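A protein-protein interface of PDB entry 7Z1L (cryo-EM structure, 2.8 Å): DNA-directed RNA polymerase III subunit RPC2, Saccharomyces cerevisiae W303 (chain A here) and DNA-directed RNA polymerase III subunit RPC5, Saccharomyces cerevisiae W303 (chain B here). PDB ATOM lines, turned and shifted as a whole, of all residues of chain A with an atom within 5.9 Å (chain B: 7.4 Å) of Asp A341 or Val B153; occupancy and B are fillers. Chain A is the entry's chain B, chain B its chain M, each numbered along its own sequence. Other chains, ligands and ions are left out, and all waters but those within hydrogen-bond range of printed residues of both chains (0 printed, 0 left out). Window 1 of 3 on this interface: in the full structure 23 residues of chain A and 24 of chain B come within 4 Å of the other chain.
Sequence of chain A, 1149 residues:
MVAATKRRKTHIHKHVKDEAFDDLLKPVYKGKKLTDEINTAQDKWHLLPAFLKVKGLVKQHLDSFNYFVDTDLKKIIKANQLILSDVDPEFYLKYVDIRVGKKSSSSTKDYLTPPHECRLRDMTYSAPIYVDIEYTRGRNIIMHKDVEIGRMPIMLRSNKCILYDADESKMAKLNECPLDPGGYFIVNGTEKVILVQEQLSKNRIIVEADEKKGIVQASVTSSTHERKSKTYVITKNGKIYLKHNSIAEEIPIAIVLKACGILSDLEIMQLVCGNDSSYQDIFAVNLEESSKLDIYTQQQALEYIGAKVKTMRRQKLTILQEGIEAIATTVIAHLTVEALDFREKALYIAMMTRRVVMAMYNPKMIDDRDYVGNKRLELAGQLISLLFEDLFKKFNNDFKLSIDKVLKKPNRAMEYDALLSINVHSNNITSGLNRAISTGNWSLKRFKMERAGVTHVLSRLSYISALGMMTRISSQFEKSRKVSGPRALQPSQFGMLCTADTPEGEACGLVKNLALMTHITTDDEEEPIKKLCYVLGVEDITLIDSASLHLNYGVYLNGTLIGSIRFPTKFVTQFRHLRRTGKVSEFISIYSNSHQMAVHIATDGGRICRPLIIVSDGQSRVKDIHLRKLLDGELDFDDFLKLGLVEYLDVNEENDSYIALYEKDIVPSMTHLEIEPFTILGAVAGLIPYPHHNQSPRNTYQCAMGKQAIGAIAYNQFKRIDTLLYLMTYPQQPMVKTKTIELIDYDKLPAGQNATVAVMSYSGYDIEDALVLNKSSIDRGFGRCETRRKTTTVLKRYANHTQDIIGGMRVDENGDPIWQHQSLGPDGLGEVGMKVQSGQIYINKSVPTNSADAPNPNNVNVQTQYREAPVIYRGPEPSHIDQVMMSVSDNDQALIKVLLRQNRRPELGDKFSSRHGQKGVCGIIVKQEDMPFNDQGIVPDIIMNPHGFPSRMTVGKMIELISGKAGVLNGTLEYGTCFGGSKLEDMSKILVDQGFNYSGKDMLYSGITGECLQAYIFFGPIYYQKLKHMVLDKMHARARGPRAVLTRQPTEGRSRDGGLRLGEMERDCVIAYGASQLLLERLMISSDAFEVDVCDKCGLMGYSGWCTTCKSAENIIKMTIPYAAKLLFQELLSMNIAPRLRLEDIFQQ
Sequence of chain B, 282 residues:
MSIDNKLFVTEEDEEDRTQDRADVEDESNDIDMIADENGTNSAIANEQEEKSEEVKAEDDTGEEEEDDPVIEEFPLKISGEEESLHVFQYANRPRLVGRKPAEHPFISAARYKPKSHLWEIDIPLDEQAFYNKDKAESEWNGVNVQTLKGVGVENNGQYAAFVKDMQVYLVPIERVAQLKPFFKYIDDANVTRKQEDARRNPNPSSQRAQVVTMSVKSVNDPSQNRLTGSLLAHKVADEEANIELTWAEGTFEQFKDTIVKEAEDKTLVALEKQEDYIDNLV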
ATOM      1  N   VAL A 337      21.845  -4.735  -2.865  1.00  0.00           N
ATOM      2  CA  VAL A 337      21.672  -3.512  -3.635  1.00  0.00           C
ATOM      3  C   VAL A 337      21.191  -2.417  -2.694  1.00  0.00           C
ATOM      4  O   VAL A 337      20.246  -2.620  -1.923  1.00  0.00           O
ATOM      5  CB  VAL A 337      20.702  -3.711  -4.817  1.00  0.00           C
ATOM      6  CG1 VAL A 337      21.392  -4.485  -5.924  1.00  0.00           C
ATOM      7  CG2 VAL A 337      19.461  -4.458  -4.379  1.00  0.00           C
ATOM      8  N   GLU A 338      21.867  -1.271  -2.732  1.00  0.00           N
ATOM      9  CA  GLU A 338      21.550  -0.141  -1.871  1.00  0.00           C
ATOM     10  C   GLU A 338      20.885   0.997  -2.629  1.00  0.00           C
ATOM     11  O   GLU A 338      20.729   2.092  -2.077  1.00  0.00           O
ATOM     12  CB  GLU A 338      22.815   0.362  -1.171  1.00  0.00           C
ATOM     13  CG  GLU A 338      23.621  -0.725  -0.474  1.00  0.00           C
ATOM     14  CD  GLU A 338      24.714  -1.300  -1.355  1.00  0.00           C
ATOM     15  OE1 GLU A 338      24.833  -0.861  -2.518  1.00  0.00           O
ATOM     16  OE2 GLU A 338      25.452  -2.191  -0.884  1.00  0.00           O
ATOM     17  N   ALA A 339      20.490   0.769  -3.875  1.00  0.00           N
ATOM     18  CA  ALA A 339      19.910   1.809  -4.714  1.00  0.00           C
ATOM     19  C   ALA A 339      18.903   1.149  -5.650  1.00  0.00           C
ATOM     20  O   ALA A 339      18.471   0.017  -5.417  1.00  0.00           O
ATOM     21  CB  ALA A 339      21.015   2.576  -5.458  1.00  0.00           C
ATOM     22  N   LEU A 340      18.524   1.858  -6.710  1.00  0.00           N
ATOM     23  CA  LEU A 340      17.529   1.358  -7.649  1.00  0.00           C
ATOM     24  C   LEU A 340      18.130   0.516  -8.765  1.00  0.00           C
ATOM     25  O   LEU A 340      17.393   0.098  -9.665  1.00  0.00           O
ATOM     26  CB  LEU A 340      16.737   2.518  -8.263  1.00  0.00           C
ATOM     27  CG  LEU A 340      15.624   3.195  -7.455  1.00  0.00           C
ATOM     28  CD1 LEU A 340      16.161   4.071  -6.333  1.00  0.00           C
ATOM     29  CD2 LEU A 340      14.719   3.993  -8.372  1.00  0.00           C
ATOM     30  N   ASP A 341      19.435   0.262  -8.741  1.00  0.00           N
ATOM     31  CA  ASP A 341      20.090  -0.514  -9.786  1.00  0.00           C
ATOM     32  C   ASP A 341      20.166  -1.978  -9.375  1.00  0.00           C
ATOM     33  O   ASP A 341      20.637  -2.300  -8.281  1.00  0.00           O
ATOM     34  CB  ASP A 341      21.491   0.030 -10.065  1.00  0.00           C
ATOM     35  CG  ASP A 341      22.124  -0.601 -11.286  1.00  0.00           C
ATOM     36  OD1 ASP A 341      21.555  -0.465 -12.389  1.00  0.00           O
ATOM     37  OD2 ASP A 341      23.192  -1.234 -11.143  1.00  0.00           O
ATOM     38  N   PHE A 342      19.706  -2.862 -10.262  1.00  0.00           N
ATOM     39  CA  PHE A 342      19.650  -4.294  -9.995  1.00  0.00           C
ATOM     40  C   PHE A 342      20.504  -5.093 -10.972  1.00  0.00           C
ATOM     41  O   PHE A 342      20.237  -6.278 -11.189  1.00  0.00           O
ATOM     42  CB  PHE A 342      18.206  -4.798 -10.048  1.00  0.00           C
ATOM     43  CG  PHE A 342      17.334  -4.302  -8.929  1.00  0.00           C
ATOM     44  CD1 PHE A 342      16.832  -3.010  -8.936  1.00  0.00           C
ATOM     45  CD2 PHE A 342      16.996  -5.137  -7.878  1.00  0.00           C
ATOM     46  CE1 PHE A 342      16.024  -2.559  -7.913  1.00  0.00           C
ATOM     47  CE2 PHE A 342      16.188  -4.691  -6.852  1.00  0.00           C
ATOM     48  CZ  PHE A 342      15.702  -3.401  -6.869  1.00  0.00           C
ATOM     49  N   ARG A 343      21.522  -4.468 -11.572  1.00  0.00           N
ATOM     50  CA  ARG A 343      22.240  -5.108 -12.672  1.00  0.00           C
ATOM     51  C   ARG A 343      23.045  -6.314 -12.204  1.00  0.00           C
ATOM     52  O   ARG A 343      23.051  -7.355 -12.870  1.00  0.00           O
ATOM     53  CB  ARG A 343      23.151  -4.098 -13.366  1.00  0.00           C
ATOM     54  CG  ARG A 343      23.625  -4.547 -14.739  1.00  0.00           C
ATOM     55  CD  ARG A 343      22.600  -4.212 -15.811  1.00  0.00           C
ATOM     56  NE  ARG A 343      22.734  -5.051 -16.996  1.00  0.00           N
ATOM     57  CZ  ARG A 343      23.637  -4.868 -17.949  1.00  0.00           C
ATOM     58  NH1 ARG A 343      24.513  -3.879 -17.893  1.00  0.00           N
ATOM     59  NH2 ARG A 343      23.657  -5.695 -18.990  1.00  0.00           N
ATOM     60  N   GLU A 344      23.737  -6.196 -11.068  1.00  0.00           N
ATOM     61  CA  GLU A 344      24.577  -7.298 -10.604  1.00  0.00           C
ATOM     62  C   GLU A 344      23.740  -8.509 -10.211  1.00  0.00           C
ATOM     63  O   GLU A 344      24.082  -9.648 -10.553  1.00  0.00           O
ATOM     64  CB  GLU A 344      25.448  -6.840  -9.435  1.00  0.00           C
ATOM     65  CG  GLU A 344      26.681  -7.702  -9.213  1.00  0.00           C
ATOM     66  CD  GLU A 344      27.688  -7.061  -8.278  1.00  0.00           C
ATOM     67  OE1 GLU A 344      27.458  -7.077  -7.052  1.00  0.00           O
ATOM     68  OE2 GLU A 344      28.711  -6.541  -8.772  1.00  0.00           O
ATOM     69  N   THR A 542      27.974  -2.568 -15.615  1.00  0.00           N
ATOM     70  CA  THR A 542      26.919  -1.571 -15.720  1.00  0.00           C
ATOM     71  C   THR A 542      26.994  -0.750 -16.999  1.00  0.00           C
ATOM     72  O   THR A 542      26.168   0.149 -17.185  1.00  0.00           O
ATOM     73  CB  THR A 542      26.959  -0.628 -14.513  1.00  0.00           C
ATOM     74  OG1 THR A 542      28.265  -0.051 -14.397  1.00  0.00           O
ATOM     75  CG2 THR A 542      26.630  -1.383 -13.237  1.00  0.00           C
ATOM     76  N   HIS B 117      18.536  10.111  -9.433  1.00  0.00           N
ATOM     77  CA  HIS B 117      19.228   9.926 -10.713  1.00  0.00           C
ATOM     78  C   HIS B 117      18.432   9.037 -11.668  1.00  0.00           C
ATOM     79  O   HIS B 117      18.992   8.199 -12.377  1.00  0.00           O
ATOM     80  CB  HIS B 117      20.642   9.380 -10.507  1.00  0.00           C
ATOM     81  CG  HIS B 117      21.419  10.106  -9.454  1.00  0.00           C
ATOM     82  ND1 HIS B 117      22.186  11.218  -9.729  1.00  0.00           N
ATOM     83  CD2 HIS B 117      21.546   9.882  -8.125  1.00  0.00           C
ATOM     84  CE1 HIS B 117      22.751  11.646  -8.615  1.00  0.00           C
ATOM     85  NE2 HIS B 117      22.381  10.853  -7.627  1.00  0.00           N
ATOM     86  N   GLY B 150      15.715   4.693 -16.861  1.00  0.00           N
ATOM     87  CA  GLY B 150      17.024   4.197 -16.487  1.00  0.00           C
ATOM     88  C   GLY B 150      17.510   4.855 -15.219  1.00  0.00           C
ATOM     89  O   GLY B 150      16.976   5.877 -14.780  1.00  0.00           O
ATOM     90  N   VAL B 151      18.533   4.251 -14.625  1.00  0.00           N
ATOM     91  CA  VAL B 151      19.178   4.772 -13.428  1.00  0.00           C
ATOM     92  C   VAL B 151      20.622   5.092 -13.775  1.00  0.00           C
ATOM     93  O   VAL B 151      21.336   4.247 -14.328  1.00  0.00           O
ATOM     94  CB  VAL B 151      19.102   3.774 -12.261  1.00  0.00           C
ATOM     95  CG1 VAL B 151      19.699   4.384 -11.004  1.00  0.00           C
ATOM     96  CG2 VAL B 151      17.664   3.346 -12.018  1.00  0.00           C
ATOM     97  N   GLY B 152      21.052   6.308 -13.455  1.00  0.00           N
ATOM     98  CA  GLY B 152      22.414   6.706 -13.743  1.00  0.00           C
ATOM     99  C   GLY B 152      23.400   6.114 -12.760  1.00  0.00           C
ATOM    100  O   GLY B 152      23.481   6.552 -11.609  1.00  0.00           O
ATOM    101  N   VAL B 153      24.157   5.118 -13.205  1.00  0.00           N
ATOM    102  CA  VAL B 153      25.131   4.459 -12.346  1.00  0.00           C
ATOM    103  C   VAL B 153      26.459   5.193 -12.456  1.00  0.00           C
ATOM    104  O   VAL B 153      26.985   5.387 -13.558  1.00  0.00           O
ATOM    105  CB  VAL B 153      25.280   2.979 -12.728  1.00  0.00           C
ATOM    106  CG1 VAL B 153      26.190   2.265 -11.740  1.00  0.00           C
ATOM    107  CG2 VAL B 153      23.917   2.309 -12.788  1.00  0.00           C
ATOM    108  N   GLU B 154      27.004   5.602 -11.315  1.00  0.00           N
ATOM    109  CA  GLU B 154      28.243   6.365 -11.289  1.00  0.00           C
ATOM    110  C   GLU B 154      29.412   5.448 -11.622  1.00  0.00           C
ATOM    111  O   GLU B 154      29.760   4.563 -10.832  1.00  0.00           O
ATOM    112  CB  GLU B 154      28.437   7.018  -9.922  1.00  0.00           C
ATOM    113  CG  GLU B 154      29.317   8.258  -9.942  1.00  0.00           C
ATOM    114  CD  GLU B 154      30.794   7.931  -9.850  1.00  0.00           C
ATOM    115  OE1 GLU B 154      31.137   6.877  -9.274  1.00  0.00           O
ATOM    116  OE2 GLU B 154      31.612   8.728 -10.356  1.00  0.00           O
ATOM    117  N   ASN B 155      30.015   5.657 -12.789  1.00  0.00           N
ATOM    118  CA  ASN B 155      31.169   4.889 -13.233  1.00  0.00           C
ATOM    119  C   ASN B 155      32.383   5.804 -13.271  1.00  0.00           C
ATOM    120  O   ASN B 155      32.334   6.881 -13.874  1.00  0.00           O
ATOM    121  CB  ASN B 155      30.926   4.267 -14.609  1.00  0.00           C
ATOM    122  CG  ASN B 155      30.264   2.908 -14.525  1.00  0.00           C
ATOM    123  OD1 ASN B 155      29.166   2.707 -15.042  1.00  0.00           O
ATOM    124  ND2 ASN B 155      30.929   1.966 -13.868  1.00  0.00           N
ATOM    125  N   ASN B 156      33.464   5.374 -12.630  1.00  0.00           N
ATOM    126  CA  ASN B 156      34.682   6.165 -12.529  1.00  0.00           C
ATOM    127  C   ASN B 156      35.683   5.730 -13.588  1.00  0.00           C
ATOM    128  O   ASN B 156      35.871   4.534 -13.828  1.00  0.00           O
ATOM    129  CB  ASN B 156      35.302   6.032 -11.138  1.00  0.00           C
ATOM    130  CG  ASN B 156      34.537   6.803 -10.083  1.00  0.00           C
ATOM    131  OD1 ASN B 156      34.452   8.029 -10.133  1.00  0.00           O
ATOM    132  ND2 ASN B 156      33.971   6.085  -9.118  1.00  0.00           N
ATOM    133  N   ILE B 173      32.862  11.627 -17.762  1.00  0.00           N
ATOM    134  CA  ILE B 173      31.477  11.178 -17.828  1.00  0.00           C
ATOM    135  C   ILE B 173      30.992  10.961 -16.404  1.00  0.00           C
ATOM    136  O   ILE B 173      31.598  10.197 -15.642  1.00  0.00           O
ATOM    137  CB  ILE B 173      31.341   9.895 -18.661  1.00  0.00           C
ATOM    138  CG1 ILE B 173      31.680  10.171 -20.124  1.00  0.00           C
ATOM    139  CG2 ILE B 173      29.939   9.332 -18.543  1.00  0.00           C
ATOM    140  CD1 ILE B 173      31.781   8.922 -20.970  1.00  0.00           C
ATOM    141  N   GLU B 174      29.902  11.635 -16.038  1.00  0.00           N
ATOM    142  CA  GLU B 174      29.396  11.532 -14.675  1.00  0.00           C
ATOM    143  C   GLU B 174      28.696  10.199 -14.447  1.00  0.00           C
ATOM    144  O   GLU B 174      29.130   9.393 -13.616  1.00  0.00           O
ATOM    145  CB  GLU B 174      28.450  12.697 -14.380  1.00  0.00           C
ATOM    146  CG  GLU B 174      28.415  13.110 -12.921  1.00  0.00           C
ATOM    147  CD  GLU B 174      27.325  14.121 -12.631  1.00  0.00           C
ATOM    148  OE1 GLU B 174      26.630  14.537 -13.580  1.00  0.00           O
ATOM    149  OE2 GLU B 174      27.164  14.501 -11.452  1.00  0.00           O
ATOM    150  N   ARG B 175      27.608   9.946 -15.173  1.00  0.00           N
ATOM    151  CA  ARG B 175      26.834   8.726 -14.993  1.00  0.00           C
ATOM    152  C   ARG B 175      26.533   8.111 -16.351  1.00  0.00           C
ATOM    153  O   ARG B 175      26.486   8.800 -17.373  1.00  0.00           O
ATOM    154  CB  ARG B 175      25.521   8.980 -14.240  1.00  0.00           C
ATOM    155  CG  ARG B 175      25.583  10.058 -13.171  1.00  0.00           C
ATOM    156  CD  ARG B 175      24.288  10.138 -12.386  1.00  0.00           C
ATOM    157  NE  ARG B 175      24.286   9.229 -11.248  1.00  0.00           N
ATOM    158  CZ  ARG B 175      24.898   9.466 -10.096  1.00  0.00           C
ATOM    159  NH1 ARG B 175      25.573  10.585  -9.889  1.00  0.00           N
ATOM    160  NH2 ARG B 175      24.830   8.559  -9.126  1.00  0.00           N
ATOM    161  N   VAL B 176      26.330   6.797 -16.346  1.00  0.00           N
ATOM    162  CA  VAL B 176      25.892   6.048 -17.518  1.00  0.00           C
ATOM    163  C   VAL B 176      24.577   5.368 -17.166  1.00  0.00           C
ATOM    164  O   VAL B 176      24.495   4.648 -16.165  1.00  0.00           O
ATOM    165  CB  VAL B 176      26.942   5.013 -17.962  1.00  0.00           C
ATOM    166  CG1 VAL B 176      26.449   4.245 -19.174  1.00  0.00           C
ATOM    167  CG2 VAL B 176      28.264   5.694 -18.264  1.00  0.00           C
ATOM    168  N   ALA B 177      23.556   5.594 -17.985  1.00  0.00           N
ATOM    169  CA  ALA B 177      22.209   5.111 -17.715  1.00  0.00           C
ATOM    170  C   ALA B 177      21.836   4.019 -18.707  1.00  0.00           C
ATOM    171  O   ALA B 177      22.007   4.190 -19.918  1.00  0.00           O
ATOM    172  CB  ALA B 177      21.195   6.254 -17.784  1.00  0.00           C
ATOM    173  N   GLN B 178      21.324   2.904 -18.191  1.00  0.00           N
ATOM    174  CA  GLN B 178      20.831   1.797 -19.008  1.00  0.00           C
ATOM    175  C   GLN B 178      19.334   2.007 -19.203  1.00  0.00           C
ATOM    176  O   GLN B 178      18.516   1.562 -18.398  1.00  0.00           O
ATOM    177  CB  GLN B 178      21.124   0.455 -18.347  1.00  0.00           C
ATOM    178  CG  GLN B 178      22.596   0.137 -18.166  1.00  0.00           C
ATOM    179  CD  GLN B 178      23.292  -0.185 -19.472  1.00  0.00           C
ATOM    180  OE1 GLN B 178      22.733  -0.860 -20.335  1.00  0.00           O
ATOM    181  NE2 GLN B 178      24.521   0.292 -19.619  1.00  0.00           N
ATOM    182  N   SER B 230      17.315  -0.363   0.151  1.00  0.00           N
ATOM    183  CA  SER B 230      16.590  -0.273  -1.113  1.00  0.00           C
ATOM    184  C   SER B 230      15.168   0.233  -0.912  1.00  0.00           C
ATOM    185  O   SER B 230      14.614   0.906  -1.788  1.00  0.00           O
ATOM    186  CB  SER B 230      16.579  -1.632  -1.810  1.00  0.00           C
ATOM    187  OG  SER B 230      15.885  -1.561  -3.042  1.00  0.00           O
ATOM    188  N   HIS B 234      13.564   3.372  -2.873  1.00  0.00           N
ATOM    189  CA  HIS B 234      12.326   3.295  -3.642  1.00  0.00           C
ATOM    190  C   HIS B 234      11.293   4.295  -3.138  1.00  0.00           C
ATOM    191  O   HIS B 234      10.583   4.915  -3.938  1.00  0.00           O
ATOM    192  CB  HIS B 234      11.765   1.873  -3.608  1.00  0.00           C
ATOM    193  CG  HIS B 234      12.429   0.943  -4.574  1.00  0.00           C
ATOM    194  ND1 HIS B 234      13.560   0.222  -4.259  1.00  0.00           N
ATOM    195  CD2 HIS B 234      12.119   0.617  -5.850  1.00  0.00           C
ATOM    196  CE1 HIS B 234      13.919  -0.507  -5.300  1.00  0.00           C
ATOM    197  NE2 HIS B 234      13.061  -0.286  -6.279  1.00  0.00           N
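OD1 of Asn B155 is in hydrogen-bond range of OG1 of Thr A542 (3.0 Å). NE2 of Gln B178 sits at hydrogen-bond distance from O of Thr A542, at 2.9 Å.
O of Val B176 is in hydrogen-bond range of N of Val B153 (3.0 Å). A ring nitrogen (ND1) of His B234 is in hydrogen-bond range of the backbone carbonyl oxygen (O) of Ser B230, at 2.8 Å.
Printed residues of chain B within 4 Å of Val A337: Ser B230. Of the printed residues of chain B, Ala A339 touches Ser B230. Printed residues of chain B within 4 Å of Leu A340: Val B151. Asp A341 touches just one residue of chain B: Val B153. Printed residues of chain A within 4 Å of Val B153: Asp A341 and Thr A542. The nearest printed residue of chain A that does not touch Val B153 is Arg A343 (6.5 Å). The nearest printed residue of chain B that does not touch Phe A342 is Ser B230 (4.3 Å).
Among the printed residues, merely in contact across the chains: Val A337 with Ser B230, Ala A339 with Ser B230, Leu A340 with Val B151, Asp A341 with Val B153, Phe A342 with His B234 and Thr A542 with Val B153.
Of the 16 printed residues of chain B, 6 touch a printed residue of chain A. Hydrophobic or aromatic side chains of chain A that line the printed part of chain B: Leu A340 and Phe A342. Among the printed residues, 8 pairs touch across the chains. Among the printed residues, no Asp or Glu carboxylate lies within 4 Å of a Lys or Arg side-chain nitrogen of the other chain.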
